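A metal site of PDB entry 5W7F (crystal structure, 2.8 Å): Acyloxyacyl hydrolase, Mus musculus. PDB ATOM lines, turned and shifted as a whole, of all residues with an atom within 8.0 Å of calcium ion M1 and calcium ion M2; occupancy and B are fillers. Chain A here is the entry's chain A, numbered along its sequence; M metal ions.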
ATOM      1  N   PRO A 168     -22.909  11.591   8.464  1.00  0.00           N
ATOM      2  CA  PRO A 168     -23.016  13.014   8.139  1.00  0.00           C
ATOM      3  C   PRO A 168     -22.587  13.293   6.714  1.00  0.00           C
ATOM      4  O   PRO A 168     -21.573  12.788   6.223  1.00  0.00           O
ATOM      5  CB  PRO A 168     -22.080  13.679   9.158  1.00  0.00           C
ATOM      6  CG  PRO A 168     -21.164  12.596   9.623  1.00  0.00           C
ATOM      7  CD  PRO A 168     -21.957  11.336   9.565  1.00  0.00           C
ATOM      8  N   LYS A 170     -21.689  16.306   5.655  1.00  0.00           N
ATOM      9  CA  LYS A 170     -20.551  17.219   5.764  1.00  0.00           C
ATOM     10  C   LYS A 170     -19.553  16.595   6.724  1.00  0.00           C
ATOM     11  O   LYS A 170     -19.684  16.732   7.947  1.00  0.00           O
ATOM     12  CB  LYS A 170     -21.007  18.594   6.244  1.00  0.00           C
ATOM     13  CG  LYS A 170     -21.984  19.305   5.327  1.00  0.00           C
ATOM     14  CD  LYS A 170     -21.285  20.046   4.196  1.00  0.00           C
ATOM     15  CE  LYS A 170     -22.272  20.832   3.346  1.00  0.00           C
ATOM     16  NZ  LYS A 170     -22.758  22.072   4.009  1.00  0.00           N
ATOM     17  N   ASP A 171     -18.544  15.908   6.186  1.00  0.00           N
ATOM     18  CA  ASP A 171     -17.571  15.221   7.024  1.00  0.00           C
ATOM     19  C   ASP A 171     -16.312  15.008   6.182  1.00  0.00           C
ATOM     20  O   ASP A 171     -16.144  13.976   5.534  1.00  0.00           O
ATOM     21  CB  ASP A 171     -18.122  13.899   7.542  1.00  0.00           C
ATOM     22  CG  ASP A 171     -17.236  13.268   8.598  1.00  0.00           C
ATOM     23  OD1 ASP A 171     -17.379  12.058   8.854  1.00  0.00           O
ATOM     24  OD2 ASP A 171     -16.408  14.000   9.183  1.00  0.00           O
ATOM     25  N   VAL A 172     -15.423  16.017   6.211  1.00  0.00           N
ATOM     26  CA  VAL A 172     -14.233  15.978   5.364  1.00  0.00           C
ATOM     27  C   VAL A 172     -13.294  14.862   5.807  1.00  0.00           C
ATOM     28  O   VAL A 172     -12.753  14.114   4.978  1.00  0.00           O
ATOM     29  CB  VAL A 172     -13.528  17.343   5.371  1.00  0.00           C
ATOM     30  CG1 VAL A 172     -12.306  17.321   4.454  1.00  0.00           C
ATOM     31  CG2 VAL A 172     -14.498  18.441   4.943  1.00  0.00           C
ATOM     32  N   ASP A 173     -13.082  14.711   7.122  1.00  0.00           N
ATOM     33  CA  ASP A 173     -12.144  13.715   7.630  1.00  0.00           C
ATOM     34  C   ASP A 173     -12.742  12.323   7.726  1.00  0.00           C
ATOM     35  O   ASP A 173     -12.010  11.373   8.008  1.00  0.00           O
ATOM     36  CB  ASP A 173     -11.621  14.141   9.005  1.00  0.00           C
ATOM     37  CG  ASP A 173     -12.725  14.317  10.032  1.00  0.00           C
ATOM     38  OD1 ASP A 173     -13.835  13.794   9.812  1.00  0.00           O
ATOM     39  OD2 ASP A 173     -12.476  14.977  11.067  1.00  0.00           O
ATOM     40  N   SER A 174     -14.060  12.187   7.522  1.00  0.00           N
ATOM     41  CA  SER A 174     -14.719  10.878   7.519  1.00  0.00           C
ATOM     42  C   SER A 174     -14.607  10.172   8.863  1.00  0.00           C
ATOM     43  O   SER A 174     -14.485   8.949   8.926  1.00  0.00           O
ATOM     44  CB  SER A 174     -14.165   9.987   6.397  1.00  0.00           C
ATOM     45  OG  SER A 174     -14.541  10.489   5.123  1.00  0.00           O
ATOM     46  N   ASP A 175     -14.630  10.938   9.960  1.00  0.00           N
ATOM     47  CA  ASP A 175     -14.744  10.370  11.294  1.00  0.00           C
ATOM     48  C   ASP A 175     -16.184  10.225  11.760  1.00  0.00           C
ATOM     49  O   ASP A 175     -16.421   9.856  12.909  1.00  0.00           O
ATOM     50  CB  ASP A 175     -13.960  11.221  12.305  1.00  0.00           C
ATOM     51  CG  ASP A 175     -14.474  12.643  12.401  1.00  0.00           C
ATOM     52  OD1 ASP A 175     -15.499  12.958  11.752  1.00  0.00           O
ATOM     53  OD2 ASP A 175     -13.860  13.436  13.135  1.00  0.00           O
ATOM     54  N   LYS A 176     -17.161  10.527  10.890  1.00  0.00           N
ATOM     55  CA  LYS A 176     -18.591  10.373  11.142  1.00  0.00           C
ATOM     56  C   LYS A 176     -19.156  11.396  12.122  1.00  0.00           C
ATOM     57  O   LYS A 176     -20.324  11.274  12.527  1.00  0.00           O
ATOM     58  CB  LYS A 176     -18.944   8.960  11.622  1.00  0.00           C
ATOM     59  CG  LYS A 176     -18.991   7.941  10.516  1.00  0.00           C
ATOM     60  CD  LYS A 176     -18.895   6.534  11.061  1.00  0.00           C
ATOM     61  CE  LYS A 176     -18.814   5.510   9.953  1.00  0.00           C
ATOM     62  NZ  LYS A 176     -18.240   4.234  10.444  1.00  0.00           N
ATOM     63  N   HIS A 177     -18.376  12.391  12.519  1.00  0.00           N
ATOM     64  CA  HIS A 177     -18.879  13.523  13.273  1.00  0.00           C
ATOM     65  C   HIS A 177     -18.712  14.777  12.419  1.00  0.00           C
ATOM     66  O   HIS A 177     -17.732  14.905  11.676  1.00  0.00           O
ATOM     67  CB  HIS A 177     -18.139  13.682  14.614  1.00  0.00           C
ATOM     68  CG  HIS A 177     -18.382  12.553  15.565  1.00  0.00           C
ATOM     69  ND1 HIS A 177     -19.016  12.714  16.775  1.00  0.00           N
ATOM     70  CD2 HIS A 177     -18.049  11.241  15.490  1.00  0.00           C
ATOM     71  CE1 HIS A 177     -19.079  11.558  17.400  1.00  0.00           C
ATOM     72  NE2 HIS A 177     -18.499  10.637  16.643  1.00  0.00           N
ATOM     73  N   SER A 178     -19.678  15.685  12.524  1.00  0.00           N
ATOM     74  CA  SER A 178     -19.761  16.821  11.615  1.00  0.00           C
ATOM     75  C   SER A 178     -19.730  18.121  12.394  1.00  0.00           C
ATOM     76  O   SER A 178     -19.923  18.162  13.609  1.00  0.00           O
ATOM     77  CB  SER A 178     -21.035  16.753  10.779  1.00  0.00           C
ATOM     78  OG  SER A 178     -21.121  17.838   9.877  1.00  0.00           O
ATOM     79  N   VAL A 179     -19.480  19.212  11.662  1.00  0.00           N
ATOM     80  CA  VAL A 179     -19.614  20.568  12.180  1.00  0.00           C
ATOM     81  C   VAL A 179     -20.934  21.204  11.773  1.00  0.00           C
ATOM     82  O   VAL A 179     -21.245  22.312  12.227  1.00  0.00           O
ATOM     83  CB  VAL A 179     -18.418  21.435  11.725  1.00  0.00           C
ATOM     84  CG1 VAL A 179     -18.534  21.794  10.243  1.00  0.00           C
ATOM     85  CG2 VAL A 179     -18.288  22.679  12.606  1.00  0.00           C
ATOM     86  N   GLY A 190     -22.143  14.099  18.828  1.00  0.00           N
ATOM     87  CA  GLY A 190     -21.383  15.244  19.287  1.00  0.00           C
ATOM     88  C   GLY A 190     -20.725  15.974  18.136  1.00  0.00           C
ATOM     89  O   GLY A 190     -20.209  15.330  17.205  1.00  0.00           O
ATOM     90  N   ARG A 191     -20.724  17.307  18.170  1.00  0.00           N
ATOM     91  CA  ARG A 191     -20.110  18.076  17.105  1.00  0.00           C
ATOM     92  C   ARG A 191     -18.608  17.847  17.074  1.00  0.00           C
ATOM     93  O   ARG A 191     -17.967  17.605  18.101  1.00  0.00           O
ATOM     94  CB  ARG A 191     -20.401  19.568  17.273  1.00  0.00           C
ATOM     95  CG  ARG A 191     -20.111  20.404  16.024  1.00  0.00           C
ATOM     96  CD  ARG A 191     -19.908  21.875  16.342  1.00  0.00           C
ATOM     97  NE  ARG A 191     -21.050  22.463  17.051  1.00  0.00           N
ATOM     98  CZ  ARG A 191     -21.837  23.430  16.581  1.00  0.00           C
ATOM     99  NH1 ARG A 191     -21.634  23.957  15.374  1.00  0.00           N
ATOM    100  NH2 ARG A 191     -22.834  23.889  17.326  1.00  0.00           N
ATOM    101  N   ASP A 192     -18.046  17.921  15.870  1.00  0.00           N
ATOM    102  CA  ASP A 192     -16.613  17.731  15.671  1.00  0.00           C
ATOM    103  C   ASP A 192     -15.911  19.077  15.752  1.00  0.00           C
ATOM    104  O   ASP A 192     -16.285  20.019  15.040  1.00  0.00           O
ATOM    105  CB  ASP A 192     -16.341  17.056  14.322  1.00  0.00           C
ATOM    106  CG  ASP A 192     -14.914  16.557  14.200  1.00  0.00           C
ATOM    107  OD1 ASP A 192     -14.188  16.546  15.218  1.00  0.00           O
ATOM    108  OD2 ASP A 192     -14.509  16.174  13.079  1.00  0.00           O
ATOM    109  N   CYS A 193     -14.911  19.165  16.622  1.00  0.00           N
ATOM    110  CA  CYS A 193     -14.168  20.410  16.789  1.00  0.00           C
ATOM    111  C   CYS A 193     -13.066  20.556  15.758  1.00  0.00           C
ATOM    112  O   CYS A 193     -12.777  21.674  15.309  1.00  0.00           O
ATOM    113  CB  CYS A 193     -13.590  20.498  18.202  1.00  0.00           C
ATOM    114  SG  CYS A 193     -12.622  19.050  18.717  1.00  0.00           S
ATOM    115  N   ASN A 194     -12.439  19.448  15.351  1.00  0.00           N
ATOM    116  CA  ASN A 194     -11.416  19.441  14.310  1.00  0.00           C
ATOM    117  C   ASN A 194     -11.909  18.551  13.176  1.00  0.00           C
ATOM    118  O   ASN A 194     -11.687  17.340  13.177  1.00  0.00           O
ATOM    119  CB  ASN A 194     -10.070  18.954  14.867  1.00  0.00           C
ATOM    120  CG  ASN A 194      -8.884  19.507  14.102  1.00  0.00           C
ATOM    121  OD1 ASN A 194      -8.993  19.888  12.934  1.00  0.00           O
ATOM    122  ND2 ASN A 194      -7.726  19.552  14.759  1.00  0.00           N
ATOM    123  N   ASP A 195     -12.608  19.157  12.211  1.00  0.00           N
ATOM    124  CA  ASP A 195     -13.121  18.402  11.070  1.00  0.00           C
ATOM    125  C   ASP A 195     -12.013  17.969  10.125  1.00  0.00           C
ATOM    126  O   ASP A 195     -12.236  17.080   9.299  1.00  0.00           O
ATOM    127  CB  ASP A 195     -14.160  19.229  10.315  1.00  0.00           C
ATOM    128  CG  ASP A 195     -15.019  18.385   9.391  1.00  0.00           C
ATOM    129  OD1 ASP A 195     -15.275  17.212   9.716  1.00  0.00           O
ATOM    130  OD2 ASP A 195     -15.433  18.904   8.334  1.00  0.00           O
ATOM    131  N   SER A 196     -10.831  18.588  10.201  1.00  0.00           N
ATOM    132  CA  SER A 196      -9.711  18.198   9.355  1.00  0.00           C
ATOM    133  C   SER A 196      -9.011  16.953   9.880  1.00  0.00           C
ATOM    134  O   SER A 196      -8.432  16.196   9.089  1.00  0.00           O
ATOM    135  CB  SER A 196      -8.711  19.347   9.242  1.00  0.00           C
ATOM    136  OG  SER A 196      -9.297  20.466   8.596  1.00  0.00           O
ATOM    137  N   ASP A 197      -9.045  16.721  11.188  1.00  0.00           N
ATOM    138  CA  ASP A 197      -8.349  15.614  11.815  1.00  0.00           C
ATOM    139  C   ASP A 197      -9.321  14.441  11.981  1.00  0.00           C
ATOM    140  O   ASP A 197     -10.344  14.572  12.666  1.00  0.00           O
ATOM    141  CB  ASP A 197      -7.773  16.039  13.168  1.00  0.00           C
ATOM    142  CG  ASP A 197      -6.678  15.121  13.652  1.00  0.00           C
ATOM    143  OD1 ASP A 197      -6.754  13.895  13.398  1.00  0.00           O
ATOM    144  OD2 ASP A 197      -5.728  15.612  14.296  1.00  0.00           O
ATOM    145  N   LYS A 198      -8.998  13.302  11.363  1.00  0.00           N
ATOM    146  CA  LYS A 198      -9.826  12.111  11.514  1.00  0.00           C
ATOM    147  C   LYS A 198      -9.532  11.348  12.800  1.00  0.00           C
ATOM    148  O   LYS A 198     -10.148  10.299  13.036  1.00  0.00           O
ATOM    149  CB  LYS A 198      -9.644  11.177  10.312  1.00  0.00           C
ATOM    150  CG  LYS A 198      -8.271  10.533  10.215  1.00  0.00           C
ATOM    151  CD  LYS A 198      -8.199   9.623   8.997  1.00  0.00           C
ATOM    152  CE  LYS A 198      -6.792   9.076   8.781  1.00  0.00           C
ATOM    153  NZ  LYS A 198      -6.721   8.187   7.584  1.00  0.00           N
ATOM    154  N   THR A 199      -8.626  11.841  13.634  1.00  0.00           N
ATOM    155  CA  THR A 199      -8.367  11.272  14.952  1.00  0.00           C
ATOM    156  C   THR A 199      -9.046  12.066  16.063  1.00  0.00           C
ATOM    157  O   THR A 199      -8.908  11.701  17.232  1.00  0.00           O
ATOM    158  CB  THR A 199      -6.856  11.205  15.226  1.00  0.00           C
ATOM    159  OG1 THR A 199      -6.363  12.515  15.550  1.00  0.00           O
ATOM    160  CG2 THR A 199      -6.108  10.661  14.017  1.00  0.00           C
ATOM    161  N   VAL A 200      -9.757  13.139  15.718  1.00  0.00           N
ATOM    162  CA  VAL A 200     -10.424  13.995  16.700  1.00  0.00           C
ATOM    163  C   VAL A 200     -11.922  13.745  16.581  1.00  0.00           C
ATOM    164  O   VAL A 200     -12.545  14.069  15.560  1.00  0.00           O
ATOM    165  CB  VAL A 200     -10.098  15.476  16.472  1.00  0.00           C
ATOM    166  CG1 VAL A 200     -10.868  16.360  17.434  1.00  0.00           C
ATOM    167  CG2 VAL A 200      -8.589  15.705  16.612  1.00  0.00           C
ATOM    168  N   TYR A 201     -12.508  13.170  17.628  1.00  0.00           N
ATOM    169  CA  TYR A 201     -13.946  12.926  17.660  1.00  0.00           C
ATOM    170  C   TYR A 201     -14.361  12.684  19.107  1.00  0.00           C
ATOM    171  O   TYR A 201     -13.558  12.154  19.893  1.00  0.00           O
ATOM    172  CB  TYR A 201     -14.318  11.714  16.789  1.00  0.00           C
ATOM    173  CG  TYR A 201     -13.551  10.457  17.107  1.00  0.00           C
ATOM    174  CD1 TYR A 201     -13.850   9.703  18.234  1.00  0.00           C
ATOM    175  CD2 TYR A 201     -12.542  10.006  16.270  1.00  0.00           C
ATOM    176  CE1 TYR A 201     -13.153   8.547  18.532  1.00  0.00           C
ATOM    177  CE2 TYR A 201     -11.837   8.849  16.557  1.00  0.00           C
ATOM    178  CZ  TYR A 201     -12.150   8.127  17.695  1.00  0.00           C
ATOM    179  OH  TYR A 201     -11.445   6.976  17.989  1.00  0.00           O
ATOM    180  N   PRO A 202     -15.578  13.061  19.499  1.00  0.00           N
ATOM    181  CA  PRO A 202     -16.020  12.798  20.867  1.00  0.00           C
ATOM    182  C   PRO A 202     -15.940  11.317  21.218  1.00  0.00           C
ATOM    183  O   PRO A 202     -16.124  10.444  20.365  1.00  0.00           O
ATOM    184  CB  PRO A 202     -17.477  13.295  20.878  1.00  0.00           C
ATOM    185  CG  PRO A 202     -17.523  14.320  19.787  1.00  0.00           C
ATOM    186  CD  PRO A 202     -16.561  13.854  18.740  1.00  0.00           C
ATOM    187  N   ASP A 214      -7.634  19.746  21.776  1.00  0.00           N
ATOM    188  CA  ASP A 214      -8.675  18.879  22.311  1.00  0.00           C
ATOM    189  C   ASP A 214      -8.851  17.653  21.409  1.00  0.00           C
ATOM    190  O   ASP A 214      -9.180  17.791  20.225  1.00  0.00           O
ATOM    191  CB  ASP A 214      -9.986  19.650  22.428  1.00  0.00           C
ATOM    192  CG  ASP A 214     -10.922  19.066  23.475  1.00  0.00           C
ATOM    193  OD1 ASP A 214     -11.833  19.785  23.919  1.00  0.00           O
ATOM    194  OD2 ASP A 214     -10.729  17.898  23.865  1.00  0.00           O
ATOM    195  N   SER A 215      -8.623  16.467  21.972  1.00  0.00           N
ATOM    196  CA  SER A 215      -8.656  15.241  21.178  1.00  0.00           C
ATOM    197  C   SER A 215     -10.078  14.714  21.011  1.00  0.00           C
ATOM    198  O   SER A 215     -10.409  14.184  19.943  1.00  0.00           O
ATOM    199  CB  SER A 215      -7.776  14.171  21.836  1.00  0.00           C
ATOM    200  OG  SER A 215      -8.235  13.866  23.146  1.00  0.00           O
ATOM    201  N   CYS A 217     -12.994  16.619  21.614  1.00  0.00           N
ATOM    202  CA  CYS A 217     -13.943  17.732  21.494  1.00  0.00           C
ATOM    203  C   CYS A 217     -14.830  17.886  22.723  1.00  0.00           C
ATOM    204  O   CYS A 217     -15.914  18.463  22.638  1.00  0.00           O
ATOM    205  CB  CYS A 217     -14.815  17.572  20.242  1.00  0.00           C
ATOM    206  SG  CYS A 217     -13.925  17.502  18.668  1.00  0.00           S
HETATM  207 CA    CA M   1     -12.444  15.143  13.567  1.00  0.00          CA
HETATM  208 CA    CA M   2     -15.377  15.189  11.149  1.00  0.00          CA
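The backbone NH (N) of Asp 192 is in hydrogen-bond range of the backbone carbonyl oxygen (O) of Ser 178.
OD1 of Asp 197 sits at hydrogen-bond distance from OG1 of Thr 199, 2.6 Å away.
A ring nitrogen (ND1) of His 177 is in hydrogen-bond range of the backbone carbonyl oxygen (O) of Gly 190 (2.9 Å).
The side-chain carboxylate of Asp 171 lies close to the backbone NH of Ser 174.
OD1 of Asp 171 sits at hydrogen-bond distance from N of Lys 176 (2.6 Å).
The side-chain sulfur of Cys 193 forms a disulfide with the side-chain sulfur of Cys 217 (2.0 Å).
Of the 27 residues printed, 6 come within 4 Å of calcium ion M1.
Within 4 Å of calcium ion M2: Asp 171, Asp 173, Asp 175, His 177, Asp 192 and Asp 195.
Calcium ion M1 is bound by the side-chain carboxylate (OD2) of Asp 175 (2.3 Å), the backbone carbonyl oxygen (O) of Val 200 (2.3 Å), the backbone carbonyl oxygen (O) of Asp 197 (2.4 Å), the backbone carbonyl oxygen (O) of Asn 194 (2.4 Å), the side-chain carboxylate (OD2) of Asp 192 (2.4 Å), the side-chain carboxylate (OD2) of Asp 173 (2.5 Å) and the side-chain carboxylate (OD1) of Asp 192 (2.8 Å).
Calcium ion M2 is bound by OD1 of Asp 175 (2.3 Å), OD2 of Asp 192 (2.3 Å), O of His 177 (2.4 Å), OD1 of Asp 173 (2.5 Å), OD1 of Asp 195 (2.5 Å) and OD2 of Asp 171 (2.5 Å).
Slightly farther from calcium ion M2 lies OD2 of Asp 173 (2.9 Å).
Slightly farther from calcium ion M2 lies the side-chain carboxylate (OD2) of Asp 175 (3.1 Å).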
